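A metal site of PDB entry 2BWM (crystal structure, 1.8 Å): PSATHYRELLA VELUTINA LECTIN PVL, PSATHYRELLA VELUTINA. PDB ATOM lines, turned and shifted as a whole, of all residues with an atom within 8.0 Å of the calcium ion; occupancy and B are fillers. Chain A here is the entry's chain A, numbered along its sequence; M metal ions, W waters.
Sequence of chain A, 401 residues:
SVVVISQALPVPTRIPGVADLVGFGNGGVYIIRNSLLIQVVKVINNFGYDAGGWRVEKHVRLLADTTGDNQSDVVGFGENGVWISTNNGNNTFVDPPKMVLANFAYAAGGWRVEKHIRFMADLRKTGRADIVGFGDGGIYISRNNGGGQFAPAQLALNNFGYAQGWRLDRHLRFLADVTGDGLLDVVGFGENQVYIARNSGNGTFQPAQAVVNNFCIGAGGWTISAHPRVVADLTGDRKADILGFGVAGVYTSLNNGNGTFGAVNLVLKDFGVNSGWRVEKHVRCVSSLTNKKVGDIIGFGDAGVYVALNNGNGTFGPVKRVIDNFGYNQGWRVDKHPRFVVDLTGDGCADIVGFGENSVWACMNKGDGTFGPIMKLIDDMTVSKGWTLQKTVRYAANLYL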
ATOM      1  N   ILE A  15      10.550 -13.974 -33.001  1.00  0.00           N
ATOM      2  CA  ILE A  15      11.333 -15.152 -33.336  1.00  0.00           C
ATOM      3  C   ILE A  15      12.571 -14.620 -34.082  1.00  0.00           C
ATOM      4  O   ILE A  15      12.408 -14.080 -35.169  1.00  0.00           O
ATOM      5  CB  ILE A  15      10.572 -16.092 -34.274  1.00  0.00           C
ATOM      6  CG1 ILE A  15       9.444 -16.807 -33.548  1.00  0.00           C
ATOM      7  CG2 ILE A  15      11.548 -17.131 -34.946  1.00  0.00           C
ATOM      8  CD1 ILE A  15       9.881 -18.089 -32.854  1.00  0.00           C
ATOM      9  N   PRO A  16      13.793 -14.726 -33.516  1.00  0.00           N
ATOM     10  CA  PRO A  16      14.154 -15.308 -32.217  1.00  0.00           C
ATOM     11  C   PRO A  16      13.812 -14.386 -31.073  1.00  0.00           C
ATOM     12  O   PRO A  16      13.690 -13.165 -31.235  1.00  0.00           O
ATOM     13  CB  PRO A  16      15.701 -15.463 -32.307  1.00  0.00           C
ATOM     14  CG  PRO A  16      16.114 -14.475 -33.256  1.00  0.00           C
ATOM     15  CD  PRO A  16      14.989 -14.241 -34.242  1.00  0.00           C
ATOM     16  N   GLY A  17      13.683 -14.981 -29.904  1.00  0.00           N
ATOM     17  CA  GLY A  17      13.457 -14.224 -28.726  1.00  0.00           C
ATOM     18  C   GLY A  17      13.537 -15.054 -27.461  1.00  0.00           C
ATOM     19  O   GLY A  17      13.522 -16.271 -27.495  1.00  0.00           O
ATOM     20  N   VAL A  18      13.523 -14.327 -26.348  1.00  0.00           N
ATOM     21  CA  VAL A  18      13.443 -14.891 -25.006  1.00  0.00           C
ATOM     22  C   VAL A  18      12.226 -14.242 -24.288  1.00  0.00           C
ATOM     23  O   VAL A  18      12.363 -13.359 -23.410  1.00  0.00           O
ATOM     24  CB  VAL A  18      14.800 -14.671 -24.195  1.00  0.00           C
ATOM     25  CG1 VAL A  18      15.895 -15.551 -24.740  1.00  0.00           C
ATOM     26  CG2 VAL A  18      15.242 -13.231 -24.220  1.00  0.00           C
ATOM     27  N   SER A 288       7.453 -21.048 -36.094  1.00  0.00           N
ATOM     28  CA  SER A 288       8.699 -21.587 -36.588  1.00  0.00           C
ATOM     29  C   SER A 288       9.402 -22.410 -35.524  1.00  0.00           C
ATOM     30  O   SER A 288       9.757 -21.878 -34.455  1.00  0.00           O
ATOM     31  CB  SER A 288       9.542 -20.391 -37.029  1.00  0.00           C
ATOM     32  OG  SER A 288      10.797 -20.804 -37.524  1.00  0.00           O
ATOM     33  N   LEU A 289       9.547 -23.717 -35.783  1.00  0.00           N
ATOM     34  CA  LEU A 289      10.171 -24.698 -34.859  1.00  0.00           C
ATOM     35  C   LEU A 289      11.591 -25.157 -35.246  1.00  0.00           C
ATOM     36  O   LEU A 289      12.178 -25.981 -34.544  1.00  0.00           O
ATOM     37  CB  LEU A 289       9.289 -25.958 -34.729  1.00  0.00           C
ATOM     38  CG  LEU A 289       7.815 -25.796 -34.336  1.00  0.00           C
ATOM     39  CD1 LEU A 289       7.091 -27.118 -34.265  1.00  0.00           C
ATOM     40  CD2 LEU A 289       7.732 -25.067 -33.092  1.00  0.00           C
ATOM     41  N   VAL A 342       6.136 -20.220 -28.356  1.00  0.00           N
ATOM     42  CA  VAL A 342       6.851 -18.941 -28.302  1.00  0.00           C
ATOM     43  C   VAL A 342       8.325 -19.273 -28.035  1.00  0.00           C
ATOM     44  O   VAL A 342       8.622 -20.225 -27.296  1.00  0.00           O
ATOM     45  CB  VAL A 342       6.271 -18.056 -27.181  1.00  0.00           C
ATOM     46  CG1 VAL A 342       6.227 -18.851 -25.859  1.00  0.00           C
ATOM     47  CG2 VAL A 342       7.010 -16.753 -27.033  1.00  0.00           C
ATOM     48  N   ASP A 343       9.229 -18.507 -28.605  1.00  0.00           N
ATOM     49  CA  ASP A 343      10.663 -18.714 -28.292  1.00  0.00           C
ATOM     50  C   ASP A 343      10.971 -18.132 -26.915  1.00  0.00           C
ATOM     51  O   ASP A 343      10.697 -16.930 -26.631  1.00  0.00           O
ATOM     52  CB  ASP A 343      11.551 -18.068 -29.374  1.00  0.00           C
ATOM     53  CG  ASP A 343      12.987 -18.603 -29.384  1.00  0.00           C
ATOM     54  OD1 ASP A 343      13.282 -19.598 -28.668  1.00  0.00           O
ATOM     55  OD2 ASP A 343      13.812 -17.993 -30.124  1.00  0.00           O
ATOM     56  N   LEU A 344      11.481 -19.036 -26.058  1.00  0.00           N
ATOM     57  CA  LEU A 344      11.857 -18.780 -24.708  1.00  0.00           C
ATOM     58  C   LEU A 344      13.399 -18.793 -24.517  1.00  0.00           C
ATOM     59  O   LEU A 344      13.885 -18.498 -23.457  1.00  0.00           O
ATOM     60  CB  LEU A 344      11.240 -19.819 -23.797  1.00  0.00           C
ATOM     61  CG  LEU A 344       9.688 -19.833 -23.746  1.00  0.00           C
ATOM     62  CD1 LEU A 344       9.230 -21.017 -22.904  1.00  0.00           C
ATOM     63  CD2 LEU A 344       9.190 -18.489 -23.190  1.00  0.00           C
ATOM     64  N   THR A 345      14.127 -19.186 -25.556  1.00  0.00           N
ATOM     65  CA  THR A 345      15.547 -19.466 -25.435  1.00  0.00           C
ATOM     66  C   THR A 345      16.460 -18.673 -26.360  1.00  0.00           C
ATOM     67  O   THR A 345      17.683 -18.732 -26.188  1.00  0.00           O
ATOM     68  CB  THR A 345      15.826 -20.956 -25.632  1.00  0.00           C
ATOM     69  OG1 THR A 345      15.628 -21.338 -26.992  1.00  0.00           O
ATOM     70  CG2 THR A 345      14.927 -21.836 -24.736  1.00  0.00           C
ATOM     71  N   GLY A 346      15.896 -17.990 -27.355  1.00  0.00           N
ATOM     72  CA  GLY A 346      16.624 -17.137 -28.257  1.00  0.00           C
ATOM     73  C   GLY A 346      17.270 -17.753 -29.470  1.00  0.00           C
ATOM     74  O   GLY A 346      17.995 -17.067 -30.213  1.00  0.00           O
ATOM     75  N   ASP A 347      17.018 -19.033 -29.723  1.00  0.00           N
ATOM     76  CA  ASP A 347      17.586 -19.737 -30.888  1.00  0.00           C
ATOM     77  C   ASP A 347      16.757 -19.623 -32.183  1.00  0.00           C
ATOM     78  O   ASP A 347      17.206 -20.085 -33.237  1.00  0.00           O
ATOM     79  CB  ASP A 347      17.904 -21.206 -30.569  1.00  0.00           C
ATOM     80  CG  ASP A 347      16.692 -22.045 -30.379  1.00  0.00           C
ATOM     81  OD1 ASP A 347      15.639 -21.449 -30.018  1.00  0.00           O
ATOM     82  OD2 ASP A 347      16.778 -23.290 -30.560  1.00  0.00           O
ATOM     83  N   GLY A 348      15.561 -19.039 -32.102  1.00  0.00           N
ATOM     84  CA  GLY A 348      14.654 -18.906 -33.245  1.00  0.00           C
ATOM     85  C   GLY A 348      13.707 -20.088 -33.472  1.00  0.00           C
ATOM     86  O   GLY A 348      12.959 -20.078 -34.459  1.00  0.00           O
ATOM     87  N   CYS A 349      13.793 -21.092 -32.594  1.00  0.00           N
ATOM     88  CA  CYS A 349      12.990 -22.316 -32.659  1.00  0.00           C
ATOM     89  C   CYS A 349      12.016 -22.232 -31.489  1.00  0.00           C
ATOM     90  O   CYS A 349      12.425 -22.286 -30.325  1.00  0.00           O
ATOM     91  CB  CYS A 349      13.887 -23.528 -32.530  1.00  0.00           C
ATOM     92  SG  CYS A 349      15.031 -23.619 -33.967  1.00  0.00           S
ATOM     93  N   ALA A 350      10.728 -22.081 -31.787  1.00  0.00           N
ATOM     94  CA  ALA A 350       9.727 -21.812 -30.754  1.00  0.00           C
ATOM     95  C   ALA A 350       9.635 -22.968 -29.768  1.00  0.00           C
ATOM     96  O   ALA A 350       9.743 -24.119 -30.136  1.00  0.00           O
ATOM     97  CB  ALA A 350       8.334 -21.473 -31.353  1.00  0.00           C
ATOM     98  N   ASP A 351       9.406 -22.609 -28.513  1.00  0.00           N
ATOM     99  CA  ASP A 351       9.260 -23.541 -27.404  1.00  0.00           C
ATOM    100  C   ASP A 351       7.781 -23.531 -26.978  1.00  0.00           C
ATOM    101  O   ASP A 351       6.967 -22.848 -27.589  1.00  0.00           O
ATOM    102  CB  ASP A 351      10.182 -23.089 -26.274  1.00  0.00           C
ATOM    103  CG  ASP A 351      11.594 -22.804 -26.779  1.00  0.00           C
ATOM    104  OD1 ASP A 351      12.217 -23.770 -27.237  1.00  0.00           O
ATOM    105  OD2 ASP A 351      12.033 -21.607 -26.774  1.00  0.00           O
ATOM    106  N   ILE A 352       7.481 -24.259 -25.918  1.00  0.00           N
ATOM    107  CA  ILE A 352       6.102 -24.369 -25.398  1.00  0.00           C
ATOM    108  C   ILE A 352       6.040 -23.896 -23.945  1.00  0.00           C
ATOM    109  O   ILE A 352       6.881 -24.241 -23.110  1.00  0.00           O
ATOM    110  CB  ILE A 352       5.546 -25.800 -25.544  1.00  0.00           C
ATOM    111  CG1 ILE A 352       5.429 -26.123 -27.006  1.00  0.00           C
ATOM    112  CG2 ILE A 352       4.141 -25.968 -24.791  1.00  0.00           C
ATOM    113  CD1 ILE A 352       5.248 -27.511 -27.297  1.00  0.00           C
ATOM    114  N   CYS A 363       8.462 -26.372 -22.073  1.00  0.00           N
ATOM    115  CA  CYS A 363       9.141 -27.467 -22.729  1.00  0.00           C
ATOM    116  C   CYS A 363       9.953 -26.908 -23.893  1.00  0.00           C
ATOM    117  O   CYS A 363       9.377 -26.244 -24.765  1.00  0.00           O
ATOM    118  CB  CYS A 363       8.112 -28.453 -23.179  1.00  0.00           C
ATOM    119  SG  CYS A 363       8.825 -29.922 -23.744  1.00  0.00           S
ATOM    120  N   MET A 364      11.281 -27.096 -23.851  1.00  0.00           N
ATOM    121  CA  MET A 364      12.147 -26.471 -24.831  1.00  0.00           C
ATOM    122  C   MET A 364      12.335 -27.282 -26.112  1.00  0.00           C
ATOM    123  O   MET A 364      12.617 -28.476 -26.108  1.00  0.00           O
ATOM    124  CB  MET A 364      13.514 -26.023 -24.214  1.00  0.00           C
ATOM    125  CG  MET A 364      13.397 -25.116 -22.954  1.00  0.00           C
ATOM    126  SD  MET A 364      12.281 -23.762 -23.071  1.00  0.00           S
ATOM    127  CE  MET A 364      12.597 -22.857 -21.588  1.00  0.00           C
ATOM    128  N   ASN A 365      12.262 -26.577 -27.229  1.00  0.00           N
ATOM    129  CA  ASN A 365      12.651 -27.106 -28.533  1.00  0.00           C
ATOM    130  C   ASN A 365      14.154 -27.389 -28.510  1.00  0.00           C
ATOM    131  O   ASN A 365      14.959 -26.532 -28.053  1.00  0.00           O
ATOM    132  CB  ASN A 365      12.340 -26.045 -29.589  1.00  0.00           C
ATOM    133  CG  ASN A 365      12.311 -26.568 -31.028  1.00  0.00           C
ATOM    134  OD1 ASN A 365      13.174 -27.323 -31.468  1.00  0.00           O
ATOM    135  ND2 ASN A 365      11.346 -26.060 -31.803  1.00  0.00           N
ATOM    136  N   LYS A 366      14.528 -28.595 -28.959  1.00  0.00           N
ATOM    137  CA  LYS A 366      15.962 -29.001 -29.082  1.00  0.00           C
ATOM    138  C   LYS A 366      16.688 -28.240 -30.184  1.00  0.00           C
ATOM    139  O   LYS A 366      17.928 -28.224 -30.224  1.00  0.00           O
ATOM    140  CB  LYS A 366      16.114 -30.527 -29.279  1.00  0.00           C
ATOM    141  CG  LYS A 366      15.629 -31.337 -28.103  1.00  0.00           C
ATOM    142  CD  LYS A 366      15.677 -32.825 -28.418  1.00  0.00           C
ATOM    143  CE  LYS A 366      15.679 -33.706 -27.189  1.00  0.00           C
ATOM    144  NZ  LYS A 366      16.033 -35.094 -27.643  1.00  0.00           N
ATOM    145  N   GLY A 367      15.927 -27.597 -31.072  1.00  0.00           N
ATOM    146  CA  GLY A 367      16.488 -26.827 -32.168  1.00  0.00           C
ATOM    147  C   GLY A 367      16.084 -27.352 -33.523  1.00  0.00           C
ATOM    148  O   GLY A 367      16.376 -26.744 -34.557  1.00  0.00           O
ATOM    149  N   PHE A 371      11.527 -32.011 -28.876  1.00  0.00           N
ATOM    150  CA  PHE A 371      11.421 -31.328 -27.595  1.00  0.00           C
ATOM    151  C   PHE A 371      12.010 -32.137 -26.435  1.00  0.00           C
ATOM    152  O   PHE A 371      11.968 -33.351 -26.482  1.00  0.00           O
ATOM    153  CB  PHE A 371       9.928 -30.987 -27.313  1.00  0.00           C
ATOM    154  CG  PHE A 371       9.430 -29.877 -28.149  1.00  0.00           C
ATOM    155  CD1 PHE A 371       9.360 -28.575 -27.650  1.00  0.00           C
ATOM    156  CD2 PHE A 371       9.046 -30.102 -29.460  1.00  0.00           C
ATOM    157  CE1 PHE A 371       8.923 -27.545 -28.439  1.00  0.00           C
ATOM    158  CE2 PHE A 371       8.577 -29.068 -30.245  1.00  0.00           C
ATOM    159  CZ  PHE A 371       8.539 -27.780 -29.714  1.00  0.00           C
HETATM  160 CA    CA M   1      13.785 -21.893 -28.476  1.00  0.00          CA
HETATM  161  O   HOH W   1      14.916 -24.070 -28.700  1.00  0.00           O
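The side-chain carboxylate of Asp 351 lies close to the backbone NH of Leu 344 (2.7 Å).
The backbone carbonyl oxygen (O) of Val 342 lies within hydrogen-bond range of the backbone NH (N) of Asp 351, at 2.8 Å.
OD2 of Asp 343 lies within hydrogen-bond range of N of Gly 17, at 3.0 Å.
The side-chain sulfur (SG) of Cys 349 lies within hydrogen-bond range of the backbone carbonyl oxygen (O) of Gly 367, at 3.5 Å.
The side-chain sulfur (SG) of Cys 349 lies close to the backbone carbonyl oxygen (O) of Leu 289, at 3.7 Å.
N of Gly 348 lies within hydrogen-bond range of OD2 of Asp 343 (2.8 Å).
The backbone NH (N) of Gly 346 sits at hydrogen-bond distance from the side-chain carboxylate (OD2) of Asp 343, 3.5 Å away.
The side-chain carboxylate (OD1) of Asp 351 sits close to the backbone NH (N) of Asn 365.
Five residues have an atom within 4 Å of the calcium ion: Asp 343, Thr 345, Asp 347, Cys 349 and Asp 351.
The nearest printed residue that does not touch the calcium ion is Leu 344 (4.4 Å).
The calcium ion is bound by O of Cys 349 (2.3 Å), OD1 of Asp 343 (2.4 Å), OG1 of Thr 345 (2.4 Å), OD1 of Asp 347 (2.5 Å), OD2 of Asp 351 (2.5 Å), water W1 (2.5 Å) and OD1 of Asp 351 (2.7 Å).
Water W1 bridges the backbone carbonyl oxygen (O) of Asn 365 (2.5 Å) and the side-chain carboxylate (OD2) of Asp 347 (2.7 Å).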
